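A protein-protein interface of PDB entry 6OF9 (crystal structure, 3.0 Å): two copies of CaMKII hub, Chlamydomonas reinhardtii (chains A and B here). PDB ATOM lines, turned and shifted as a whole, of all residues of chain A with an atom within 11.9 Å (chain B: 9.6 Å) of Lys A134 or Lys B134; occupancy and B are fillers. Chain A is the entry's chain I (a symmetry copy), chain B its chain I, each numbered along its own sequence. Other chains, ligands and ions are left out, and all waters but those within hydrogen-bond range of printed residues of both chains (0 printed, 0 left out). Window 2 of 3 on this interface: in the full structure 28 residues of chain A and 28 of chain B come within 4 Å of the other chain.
The side-chain amide nitrogen (NE2) of Gln B109 sits at hydrogen-bond distance from the backbone carbonyl oxygen (O) of Lys B134 (3.5 Å).
The side-chain hydroxyl (OG) of Ser A131 lies within hydrogen-bond range of the side-chain carboxylate (OE1) of Glu A111 (2.6 Å).
The backbone carbonyl oxygen (O) of Gln A109 lies within hydrogen-bond range of the backbone NH (N) of Val A133 (3.4 Å).
The side-chain amide nitrogen (NE2) of Gln A109 is in hydrogen-bond range of the backbone carbonyl oxygen (O) of Lys A134.
The backbone carbonyl oxygen (O) of Gln B109 lies within hydrogen-bond range of the backbone NH (N) of Val B133 (3.4 Å).
OE1 of Glu B111 sits at hydrogen-bond distance from OG of Ser B131 (2.6 Å).
Among the printed residues, pairs that only touch across the chains: Glu A111 with Gly B43 (3.3 Å), Gly A43 with Glu B111 (3.3 Å), His A129 with Ser B131 (3.4 Å), Ser A131 with Ser B131 (3.5 Å), His A129 with Glu B111 (3.6 Å), Lys A134 with Lys B134 (3.8 Å), His A44 with Glu B111 (3.8 Å), Glu A111 with His B44 (3.8 Å), Gly A43 with Val B133 (3.9 Å), Val A133 with Gly B43 (3.9 Å) and Ile A94 with Gly B43 (3.98 Å).
Of the 13 printed residues of chain B, 6 touch a printed residue of chain A.
Hydrophobic or aromatic side chains of chain B that line the printed part of chain A: Val B133.
Of the 23 printed residues of chain A, 8 touch a printed residue of chain B.
Hydrophobic or aromatic side chains of chain A within 4 Å of the printed part of chain B: Ile A94, His A129 and Val A133.
Gly A43 touches Glu B111, and with the chains exchanged Glu A111 touches Gly B43.
Gly A43 touches Val B133, and with the chains exchanged Val A133 touches Gly B43.
His A44 touches Glu B111, and with the chains exchanged Glu A111 touches His B44.
Lys B134 touches its own counterpart, Lys A134.
Positions printed for both chains: 39, 42, 43, 44, 107, 108, 109, 110, 111, 131, 132, 133 and 134.
Of the 11 pairs that touch across the chains among the printed residues, 8 have their exchanged pair printed and touching as well.
Lys A134 touches one residue of chain B.
Lys B134 touches one residue of chain A.
Printed residues of chain B within 4 Å of Val A133: Gly B43.
No residue of chain A comes within 4 Å of Leu B132.
Val B133 touches just one residue of chain A: Gly A43 (3.9 Å).
Of the printed residues of chain B, Ser A131 touches Ser B131 (3.5 Å).
Of the printed residues of chain A, Glu B111 touches Gly A43 (3.3 Å), His A44 (3.8 Å) and His A129 (3.6 Å).
Of the printed residues of chain B, Glu A111 touches Gly B43 (3.3 Å) and His B44 (3.8 Å).
Of the printed residues of chain A, Ser B131 touches His A129 (3.4 Å) and Ser A131 (3.5 Å).
Printed residues of chain B within 4 Å of Ile A94: Gly B43 (3.98 Å).
Arg A130 touches none of the printed residues of chain B.
Val A42 touches none of the printed residues of chain B.
The nearest residue of chain A that does not touch Lys B134 is Leu A132 (6.5 Å).
The nearest printed residue of chain A that does not touch His B44 is Ile A94 (4.6 Å).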
ATOM      1  N   GLU A  38      21.767  -8.998 -28.293  1.00  0.00           N
ATOM      2  CA  GLU A  38      22.750  -9.375 -27.286  1.00  0.00           C
ATOM      3  C   GLU A  38      23.965  -8.469 -27.433  1.00  0.00           C
ATOM      4  O   GLU A  38      24.145  -7.836 -28.480  1.00  0.00           O
ATOM      5  CB  GLU A  38      23.141 -10.860 -27.411  1.00  0.00           C
ATOM      6  CG  GLU A  38      24.085 -11.210 -28.547  1.00  0.00           C
ATOM      7  CD  GLU A  38      24.474 -12.682 -28.528  1.00  0.00           C
ATOM      8  OE1 GLU A  38      25.510 -13.041 -29.126  1.00  0.00           O
ATOM      9  OE2 GLU A  38      23.743 -13.481 -27.908  1.00  0.00           O
ATOM     10  N   PRO A  39      24.802  -8.366 -26.393  1.00  0.00           N
ATOM     11  CA  PRO A  39      25.975  -7.478 -26.483  1.00  0.00           C
ATOM     12  C   PRO A  39      26.910  -7.808 -27.632  1.00  0.00           C
ATOM     13  O   PRO A  39      27.506  -6.896 -28.217  1.00  0.00           O
ATOM     14  CB  PRO A  39      26.661  -7.677 -25.125  1.00  0.00           C
ATOM     15  CG  PRO A  39      25.577  -8.110 -24.214  1.00  0.00           C
ATOM     16  CD  PRO A  39      24.657  -8.946 -25.046  1.00  0.00           C
ATOM     17  N   GLU A  40      27.060  -9.089 -27.972  1.00  0.00           N
ATOM     18  CA  GLU A  40      27.929  -9.469 -29.078  1.00  0.00           C
ATOM     19  C   GLU A  40      27.391  -9.001 -30.425  1.00  0.00           C
ATOM     20  O   GLU A  40      28.149  -8.954 -31.400  1.00  0.00           O
ATOM     21  CB  GLU A  40      28.125 -10.988 -29.087  1.00  0.00           C
ATOM     22  CG  GLU A  40      28.835 -11.546 -27.856  1.00  0.00           C
ATOM     23  CD  GLU A  40      27.904 -11.756 -26.669  1.00  0.00           C
ATOM     24  OE1 GLU A  40      26.784 -11.199 -26.674  1.00  0.00           O
ATOM     25  OE2 GLU A  40      28.291 -12.483 -25.730  1.00  0.00           O
ATOM     26  N   ALA A  41      26.107  -8.651 -30.501  1.00  0.00           N
ATOM     27  CA  ALA A  41      25.491  -8.142 -31.720  1.00  0.00           C
ATOM     28  C   ALA A  41      25.680  -6.639 -31.898  1.00  0.00           C
ATOM     29  O   ALA A  41      25.051  -6.059 -32.790  1.00  0.00           O
ATOM     30  CB  ALA A  41      24.000  -8.485 -31.736  1.00  0.00           C
ATOM     31  N   VAL A  42      26.537  -6.024 -31.076  1.00  0.00           N
ATOM     32  CA  VAL A  42      26.906  -4.606 -31.094  1.00  0.00           C
ATOM     33  C   VAL A  42      25.765  -3.696 -31.540  1.00  0.00           C
ATOM     34  O   VAL A  42      25.939  -2.843 -32.418  1.00  0.00           O
ATOM     35  CB  VAL A  42      28.169  -4.372 -31.952  1.00  0.00           C
ATOM     36  CG1 VAL A  42      29.392  -4.961 -31.259  1.00  0.00           C
ATOM     37  CG2 VAL A  42      28.023  -4.949 -33.359  1.00  0.00           C
ATOM     38  N   GLY A  43      24.596  -3.859 -30.925  1.00  0.00           N
ATOM     39  CA  GLY A  43      23.502  -2.930 -31.129  1.00  0.00           C
ATOM     40  C   GLY A  43      22.628  -3.192 -32.332  1.00  0.00           C
ATOM     41  O   GLY A  43      22.001  -2.256 -32.838  1.00  0.00           O
ATOM     42  N   HIS A  44      22.557  -4.433 -32.805  1.00  0.00           N
ATOM     43  CA  HIS A  44      21.737  -4.774 -33.958  1.00  0.00           C
ATOM     44  C   HIS A  44      20.967  -6.055 -33.668  1.00  0.00           C
ATOM     45  O   HIS A  44      21.302  -6.813 -32.754  1.00  0.00           O
ATOM     46  CB  HIS A  44      22.588  -4.936 -35.226  1.00  0.00           C
ATOM     47  CG  HIS A  44      23.437  -3.743 -35.537  1.00  0.00           C
ATOM     48  ND1 HIS A  44      22.917  -2.570 -36.044  1.00  0.00           N
ATOM     49  CD2 HIS A  44      24.769  -3.539 -35.410  1.00  0.00           C
ATOM     50  CE1 HIS A  44      23.893  -1.697 -36.216  1.00  0.00           C
ATOM     51  NE2 HIS A  44      25.027  -2.259 -35.838  1.00  0.00           N
ATOM     52  N   ILE A  94      17.053 -12.218 -14.348  1.00  0.00           N
ATOM     53  CA  ILE A  94      18.410 -11.689 -14.313  1.00  0.00           C
ATOM     54  C   ILE A  94      19.355 -12.884 -14.317  1.00  0.00           C
ATOM     55  O   ILE A  94      19.394 -13.662 -13.360  1.00  0.00           O
ATOM     56  CB  ILE A  94      18.651 -10.784 -13.096  1.00  0.00           C
ATOM     57  CG1 ILE A  94      17.820  -9.500 -13.201  1.00  0.00           C
ATOM     58  CG2 ILE A  94      20.124 -10.436 -12.976  1.00  0.00           C
ATOM     59  CD1 ILE A  94      16.420  -9.615 -12.628  1.00  0.00           C
ATOM     60  N   ARG A  95      20.094 -13.051 -15.405  1.00  0.00           N
ATOM     61  CA  ARG A  95      21.060 -14.134 -15.506  1.00  0.00           C
ATOM     62  C   ARG A  95      22.325 -13.752 -14.748  1.00  0.00           C
ATOM     63  O   ARG A  95      22.945 -12.722 -15.042  1.00  0.00           O
ATOM     64  CB  ARG A  95      21.369 -14.434 -16.970  1.00  0.00           C
ATOM     65  CG  ARG A  95      22.386 -15.538 -17.183  1.00  0.00           C
ATOM     66  CD  ARG A  95      22.484 -15.883 -18.654  1.00  0.00           C
ATOM     67  NE  ARG A  95      23.599 -16.777 -18.942  1.00  0.00           N
ATOM     68  CZ  ARG A  95      23.971 -17.129 -20.168  1.00  0.00           C
ATOM     69  NH1 ARG A  95      23.313 -16.660 -21.220  1.00  0.00           N
ATOM     70  NH2 ARG A  95      25.000 -17.949 -20.343  1.00  0.00           N
ATOM     71  N   LEU A  96      22.689 -14.575 -13.762  1.00  0.00           N
ATOM     72  CA  LEU A  96      23.926 -14.436 -13.001  1.00  0.00           C
ATOM     73  C   LEU A  96      24.841 -15.589 -13.394  1.00  0.00           C
ATOM     74  O   LEU A  96      24.539 -16.752 -13.110  1.00  0.00           O
ATOM     75  CB  LEU A  96      23.656 -14.444 -11.497  1.00  0.00           C
ATOM     76  CG  LEU A  96      22.812 -13.312 -10.914  1.00  0.00           C
ATOM     77  CD1 LEU A  96      22.639 -13.506  -9.419  1.00  0.00           C
ATOM     78  CD2 LEU A  96      23.446 -11.965 -11.205  1.00  0.00           C
ATOM     79  N   VAL A 106      34.165 -14.463 -10.426  1.00  0.00           N
ATOM     80  CA  VAL A 106      33.415 -13.246 -10.702  1.00  0.00           C
ATOM     81  C   VAL A 106      31.998 -13.621 -11.111  1.00  0.00           C
ATOM     82  O   VAL A 106      31.750 -14.690 -11.685  1.00  0.00           O
ATOM     83  CB  VAL A 106      34.076 -12.372 -11.793  1.00  0.00           C
ATOM     84  CG1 VAL A 106      35.444 -11.873 -11.339  1.00  0.00           C
ATOM     85  CG2 VAL A 106      34.177 -13.136 -13.098  1.00  0.00           C
ATOM     86  N   THR A 107      31.064 -12.723 -10.810  1.00  0.00           N
ATOM     87  CA  THR A 107      29.652 -12.893 -11.125  1.00  0.00           C
ATOM     88  C   THR A 107      29.245 -11.832 -12.139  1.00  0.00           C
ATOM     89  O   THR A 107      29.360 -10.632 -11.867  1.00  0.00           O
ATOM     90  CB  THR A 107      28.792 -12.787  -9.865  1.00  0.00           C
ATOM     91  OG1 THR A 107      29.234 -13.749  -8.898  1.00  0.00           O
ATOM     92  CG2 THR A 107      27.328 -13.042 -10.195  1.00  0.00           C
ATOM     93  N   VAL A 108      28.778 -12.277 -13.302  1.00  0.00           N
ATOM     94  CA  VAL A 108      28.293 -11.403 -14.364  1.00  0.00           C
ATOM     95  C   VAL A 108      26.774 -11.371 -14.309  1.00  0.00           C
ATOM     96  O   VAL A 108      26.128 -12.413 -14.149  1.00  0.00           O
ATOM     97  CB  VAL A 108      28.791 -11.884 -15.739  1.00  0.00           C
ATOM     98  CG1 VAL A 108      28.012 -11.217 -16.864  1.00  0.00           C
ATOM     99  CG2 VAL A 108      30.281 -11.617 -15.883  1.00  0.00           C
ATOM    100  N   GLN A 109      26.197 -10.179 -14.432  1.00  0.00           N
ATOM    101  CA  GLN A 109      24.752 -10.009 -14.415  1.00  0.00           C
ATOM    102  C   GLN A 109      24.273  -9.499 -15.767  1.00  0.00           C
ATOM    103  O   GLN A 109      24.937  -8.673 -16.403  1.00  0.00           O
ATOM    104  CB  GLN A 109      24.316  -9.046 -13.305  1.00  0.00           C
ATOM    105  CG  GLN A 109      25.061  -7.724 -13.282  1.00  0.00           C
ATOM    106  CD  GLN A 109      24.668  -6.857 -12.100  1.00  0.00           C
ATOM    107  OE1 GLN A 109      23.521  -6.878 -11.653  1.00  0.00           O
ATOM    108  NE2 GLN A 109      25.625  -6.095 -11.582  1.00  0.00           N
ATOM    109  N   ALA A 110      23.124 -10.007 -16.207  1.00  0.00           N
ATOM    110  CA  ALA A 110      22.519  -9.535 -17.445  1.00  0.00           C
ATOM    111  C   ALA A 110      21.004  -9.631 -17.343  1.00  0.00           C
ATOM    112  O   ALA A 110      20.475 -10.570 -16.749  1.00  0.00           O
ATOM    113  CB  ALA A 110      23.017 -10.337 -18.651  1.00  0.00           C
ATOM    114  N   GLU A 111      20.308  -8.649 -17.914  1.00  0.00           N
ATOM    115  CA  GLU A 111      18.860  -8.733 -18.057  1.00  0.00           C
ATOM    116  C   GLU A 111      18.535  -9.620 -19.252  1.00  0.00           C
ATOM    117  O   GLU A 111      19.045  -9.388 -20.353  1.00  0.00           O
ATOM    118  CB  GLU A 111      18.256  -7.341 -18.248  1.00  0.00           C
ATOM    119  CG  GLU A 111      18.598  -6.345 -17.149  1.00  0.00           C
ATOM    120  CD  GLU A 111      18.227  -4.915 -17.509  1.00  0.00           C
ATOM    121  OE1 GLU A 111      18.432  -4.522 -18.677  1.00  0.00           O
ATOM    122  OE2 GLU A 111      17.729  -4.183 -16.625  1.00  0.00           O
ATOM    123  N   GLU A 112      17.700 -10.642 -19.048  1.00  0.00           N
ATOM    124  CA  GLU A 112      17.398 -11.576 -20.126  1.00  0.00           C
ATOM    125  C   GLU A 112      15.897 -11.764 -20.273  1.00  0.00           C
ATOM    126  O   GLU A 112      15.197 -12.065 -19.297  1.00  0.00           O
ATOM    127  CB  GLU A 112      18.079 -12.931 -19.902  1.00  0.00           C
ATOM    128  CG  GLU A 112      19.557 -12.934 -20.270  1.00  0.00           C
ATOM    129  CD  GLU A 112      20.073 -14.316 -20.636  1.00  0.00           C
ATOM    130  OE1 GLU A 112      19.281 -15.282 -20.593  1.00  0.00           O
ATOM    131  OE2 GLU A 112      21.269 -14.435 -20.976  1.00  0.00           O
ATOM    132  N   HIS A 129      16.626 -11.573 -25.866  1.00  0.00           N
ATOM    133  CA  HIS A 129      17.014 -10.180 -25.652  1.00  0.00           C
ATOM    134  C   HIS A 129      17.850 -10.111 -24.381  1.00  0.00           C
ATOM    135  O   HIS A 129      17.331 -10.313 -23.279  1.00  0.00           O
ATOM    136  CB  HIS A 129      15.791  -9.267 -25.561  1.00  0.00           C
ATOM    137  CG  HIS A 129      16.124  -7.806 -25.582  1.00  0.00           C
ATOM    138  ND1 HIS A 129      17.414  -7.333 -25.483  1.00  0.00           N
ATOM    139  CD2 HIS A 129      15.331  -6.713 -25.689  1.00  0.00           C
ATOM    140  CE1 HIS A 129      17.403  -6.012 -25.526  1.00  0.00           C
ATOM    141  NE2 HIS A 129      16.151  -5.611 -25.650  1.00  0.00           N
ATOM    142  N   ARG A 130      19.136  -9.804 -24.537  1.00  0.00           N
ATOM    143  CA  ARG A 130      20.108  -9.829 -23.454  1.00  0.00           C
ATOM    144  C   ARG A 130      20.807  -8.481 -23.377  1.00  0.00           C
ATOM    145  O   ARG A 130      21.262  -7.954 -24.398  1.00  0.00           O
ATOM    146  CB  ARG A 130      21.124 -10.955 -23.682  1.00  0.00           C
ATOM    147  CG  ARG A 130      22.101 -11.187 -22.547  1.00  0.00           C
ATOM    148  CD  ARG A 130      22.875 -12.480 -22.769  1.00  0.00           C
ATOM    149  NE  ARG A 130      24.306 -12.250 -22.947  1.00  0.00           N
ATOM    150  CZ  ARG A 130      25.188 -12.237 -21.952  1.00  0.00           C
ATOM    151  NH1 ARG A 130      26.472 -12.021 -22.203  1.00  0.00           N
ATOM    152  NH2 ARG A 130      24.783 -12.442 -20.704  1.00  0.00           N
ATOM    153  N   SER A 131      20.889  -7.923 -22.171  1.00  0.00           N
ATOM    154  CA  SER A 131      21.536  -6.635 -21.951  1.00  0.00           C
ATOM    155  C   SER A 131      22.397  -6.708 -20.701  1.00  0.00           C
ATOM    156  O   SER A 131      21.929  -7.145 -19.646  1.00  0.00           O
ATOM    157  CB  SER A 131      20.503  -5.512 -21.813  1.00  0.00           C
ATOM    158  OG  SER A 131      19.683  -5.705 -20.675  1.00  0.00           O
ATOM    159  N   LEU A 132      23.648  -6.270 -20.818  1.00  0.00           N
ATOM    160  CA  LEU A 132      24.572  -6.318 -19.696  1.00  0.00           C
ATOM    161  C   LEU A 132      24.322  -5.169 -18.729  1.00  0.00           C
ATOM    162  O   LEU A 132      24.096  -4.026 -19.137  1.00  0.00           O
ATOM    163  CB  LEU A 132      26.020  -6.275 -20.185  1.00  0.00           C
ATOM    164  CG  LEU A 132      26.632  -7.599 -20.643  1.00  0.00           C
ATOM    165  CD1 LEU A 132      28.074  -7.394 -21.080  1.00  0.00           C
ATOM    166  CD2 LEU A 132      26.548  -8.641 -19.540  1.00  0.00           C
ATOM    167  N   VAL A 133      24.364  -5.486 -17.438  1.00  0.00           N
ATOM    168  CA  VAL A 133      24.303  -4.501 -16.367  1.00  0.00           C
ATOM    169  C   VAL A 133      25.676  -4.432 -15.713  1.00  0.00           C
ATOM    170  O   VAL A 133      26.307  -5.466 -15.465  1.00  0.00           O
ATOM    171  CB  VAL A 133      23.214  -4.855 -15.335  1.00  0.00           C
ATOM    172  CG1 VAL A 133      23.112  -3.773 -14.270  1.00  0.00           C
ATOM    173  CG2 VAL A 133      21.876  -5.065 -16.025  1.00  0.00           C
ATOM    174  N   LYS A 134      26.143  -3.216 -15.450  1.00  0.00           N
ATOM    175  CA  LYS A 134      27.440  -3.027 -14.807  1.00  0.00           C
ATOM    176  C   LYS A 134      27.277  -2.361 -13.445  1.00  0.00           C
ATOM    177  O   LYS A 134      26.606  -2.891 -12.560  1.00  0.00           O
ATOM    178  CB  LYS A 134      28.376  -2.194 -15.690  1.00  0.00           C
ATOM    179  CG  LYS A 134      28.836  -2.885 -16.970  1.00  0.00           C
ATOM    180  CD  LYS A 134      27.850  -2.672 -18.109  1.00  0.00           C
ATOM    181  CE  LYS A 134      27.654  -1.192 -18.395  1.00  0.00           C
ATOM    182  NZ  LYS A 134      26.618  -0.960 -19.439  1.00  0.00           N
ATOM    183  N   PRO B  39      16.565   0.944 -18.790  1.00  0.00           N
ATOM    184  CA  PRO B  39      17.687   1.567 -18.065  1.00  0.00           C
ATOM    185  C   PRO B  39      17.280   2.246 -16.769  1.00  0.00           C
ATOM    186  O   PRO B  39      18.054   2.235 -15.805  1.00  0.00           O
ATOM    187  CB  PRO B  39      18.234   2.578 -19.081  1.00  0.00           C
ATOM    188  CG  PRO B  39      17.839   2.036 -20.401  1.00  0.00           C
ATOM    189  CD  PRO B  39      16.506   1.390 -20.193  1.00  0.00           C
ATOM    190  N   VAL B  42      17.452   0.329 -13.380  1.00  0.00           N
ATOM    191  CA  VAL B  42      18.802   0.042 -12.887  1.00  0.00           C
ATOM    192  C   VAL B  42      19.061  -1.448 -12.684  1.00  0.00           C
ATOM    193  O   VAL B  42      19.540  -1.871 -11.626  1.00  0.00           O
ATOM    194  CB  VAL B  42      19.101   0.837 -11.596  1.00  0.00           C
ATOM    195  CG1 VAL B  42      19.238   2.322 -11.912  1.00  0.00           C
ATOM    196  CG2 VAL B  42      18.034   0.615 -10.524  1.00  0.00           C
ATOM    197  N   GLY B  43      18.766  -2.249 -13.705  1.00  0.00           N
ATOM    198  CA  GLY B  43      19.147  -3.648 -13.699  1.00  0.00           C
ATOM    199  C   GLY B  43      18.194  -4.589 -13.001  1.00  0.00           C
ATOM    200  O   GLY B  43      18.621  -5.657 -12.551  1.00  0.00           O
ATOM    201  N   HIS B  44      16.915  -4.237 -12.902  1.00  0.00           N
ATOM    202  CA  HIS B  44      15.929  -5.085 -12.250  1.00  0.00           C
ATOM    203  C   HIS B  44      14.669  -5.141 -13.102  1.00  0.00           C
ATOM    204  O   HIS B  44      14.451  -4.306 -13.983  1.00  0.00           O
ATOM    205  CB  HIS B  44      15.599  -4.580 -10.837  1.00  0.00           C
ATOM    206  CG  HIS B  44      16.801  -4.423  -9.958  1.00  0.00           C
ATOM    207  ND1 HIS B  44      17.468  -5.498  -9.410  1.00  0.00           N
ATOM    208  CD2 HIS B  44      17.457  -3.317  -9.535  1.00  0.00           C
ATOM    209  CE1 HIS B  44      18.484  -5.060  -8.687  1.00  0.00           C
ATOM    210  NE2 HIS B  44      18.499  -3.741  -8.746  1.00  0.00           N
ATOM    211  N   THR B 107      20.511  12.023 -31.546  1.00  0.00           N
ATOM    212  CA  THR B 107      19.789  10.789 -31.822  1.00  0.00           C
ATOM    213  C   THR B 107      20.210   9.737 -30.804  1.00  0.00           C
ATOM    214  O   THR B 107      21.394   9.392 -30.715  1.00  0.00           O
ATOM    215  CB  THR B 107      20.065  10.298 -33.244  1.00  0.00           C
ATOM    216  OG1 THR B 107      19.724  11.326 -34.182  1.00  0.00           O
ATOM    217  CG2 THR B 107      19.248   9.050 -33.545  1.00  0.00           C
ATOM    218  N   VAL B 108      19.245   9.238 -30.038  1.00  0.00           N
ATOM    219  CA  VAL B 108      19.460   8.186 -29.050  1.00  0.00           C
ATOM    220  C   VAL B 108      19.015   6.861 -29.649  1.00  0.00           C
ATOM    221  O   VAL B 108      17.957   6.780 -30.281  1.00  0.00           O
ATOM    222  CB  VAL B 108      18.697   8.494 -27.748  1.00  0.00           C
ATOM    223  CG1 VAL B 108      18.614   7.258 -26.862  1.00  0.00           C
ATOM    224  CG2 VAL B 108      19.361   9.644 -27.008  1.00  0.00           C
ATOM    225  N   GLN B 109      19.823   5.821 -29.462  1.00  0.00           N
ATOM    226  CA  GLN B 109      19.509   4.492 -29.966  1.00  0.00           C
ATOM    227  C   GLN B 109      19.303   3.532 -28.804  1.00  0.00           C
ATOM    228  O   GLN B 109      20.005   3.606 -27.790  1.00  0.00           O
ATOM    229  CB  GLN B 109      20.615   3.971 -30.891  1.00  0.00           C
ATOM    230  CG  GLN B 109      22.018   4.063 -30.318  1.00  0.00           C
ATOM    231  CD  GLN B 109      23.079   3.637 -31.315  1.00  0.00           C
ATOM    232  OE1 GLN B 109      22.853   2.754 -32.143  1.00  0.00           O
ATOM    233  NE2 GLN B 109      24.244   4.272 -31.246  1.00  0.00           N
ATOM    234  N   ALA B 110      18.326   2.640 -28.953  1.00  0.00           N
ATOM    235  CA  ALA B 110      18.087   1.612 -27.949  1.00  0.00           C
ATOM    236  C   ALA B 110      17.550   0.356 -28.619  1.00  0.00           C
ATOM    237  O   ALA B 110      16.777   0.438 -29.574  1.00  0.00           O
ATOM    238  CB  ALA B 110      17.107   2.096 -26.876  1.00  0.00           C
ATOM    239  N   GLU B 111      17.971  -0.806 -28.124  1.00  0.00           N
ATOM    240  CA  GLU B 111      17.376  -2.068 -28.547  1.00  0.00           C
ATOM    241  C   GLU B 111      16.060  -2.262 -27.806  1.00  0.00           C
ATOM    242  O   GLU B 111      16.024  -2.182 -26.575  1.00  0.00           O
ATOM    243  CB  GLU B 111      18.325  -3.233 -28.260  1.00  0.00           C
ATOM    244  CG  GLU B 111      19.707  -3.094 -28.882  1.00  0.00           C
ATOM    245  CD  GLU B 111      20.701  -4.113 -28.349  1.00  0.00           C
ATOM    246  OE1 GLU B 111      20.682  -4.384 -27.130  1.00  0.00           O
ATOM    247  OE2 GLU B 111      21.502  -4.646 -29.149  1.00  0.00           O
ATOM    248  N   SER B 131      17.232  -1.637 -23.911  1.00  0.00           N
ATOM    249  CA  SER B 131      18.645  -1.568 -23.560  1.00  0.00           C
ATOM    250  C   SER B 131      19.319  -0.484 -24.385  1.00  0.00           C
ATOM    251  O   SER B 131      19.173  -0.452 -25.610  1.00  0.00           O
ATOM    252  CB  SER B 131      19.340  -2.914 -23.792  1.00  0.00           C
ATOM    253  OG  SER B 131      19.323  -3.272 -25.162  1.00  0.00           O
ATOM    254  N   LEU B 132      20.063   0.392 -23.716  1.00  0.00           N
ATOM    255  CA  LEU B 132      20.732   1.489 -24.397  1.00  0.00           C
ATOM    256  C   LEU B 132      22.009   1.015 -25.079  1.00  0.00           C
ATOM    257  O   LEU B 132      22.782   0.233 -24.519  1.00  0.00           O
ATOM    258  CB  LEU B 132      21.060   2.615 -23.415  1.00  0.00           C
ATOM    259  CG  LEU B 132      19.936   3.602 -23.099  1.00  0.00           C
ATOM    260  CD1 LEU B 132      20.422   4.666 -22.128  1.00  0.00           C
ATOM    261  CD2 LEU B 132      19.405   4.238 -24.373  1.00  0.00           C
ATOM    262  N   VAL B 133      22.219   1.499 -26.300  1.00  0.00           N
ATOM    263  CA  VAL B 133      23.450   1.285 -27.047  1.00  0.00           C
ATOM    264  C   VAL B 133      24.196   2.610 -27.114  1.00  0.00           C
ATOM    265  O   VAL B 133      23.590   3.662 -27.355  1.00  0.00           O
ATOM    266  CB  VAL B 133      23.167   0.735 -28.459  1.00  0.00           C
ATOM    267  CG1 VAL B 133      24.468   0.443 -29.191  1.00  0.00           C
ATOM    268  CG2 VAL B 133      22.298  -0.509 -28.381  1.00  0.00           C
ATOM    269  N   LYS B 134      25.504   2.564 -26.885  1.00  0.00           N
ATOM    270  CA  LYS B 134      26.325   3.769 -26.942  1.00  0.00           C
ATOM    271  C   LYS B 134      27.353   3.673 -28.064  1.00  0.00           C
ATOM    272  O   LYS B 134      26.997   3.527 -29.234  1.00  0.00           O
ATOM    273  CB  LYS B 134      27.031   4.018 -25.604  1.00  0.00           C
ATOM    274  CG  LYS B 134      26.107   4.404 -24.452  1.00  0.00           C
ATOM    275  CD  LYS B 134      25.556   3.179 -23.739  1.00  0.00           C
ATOM    276  CE  LYS B 134      26.679   2.308 -23.196  1.00  0.00           C
ATOM    277  NZ  LYS B 134      26.162   1.054 -22.582  1.00  0.00           N
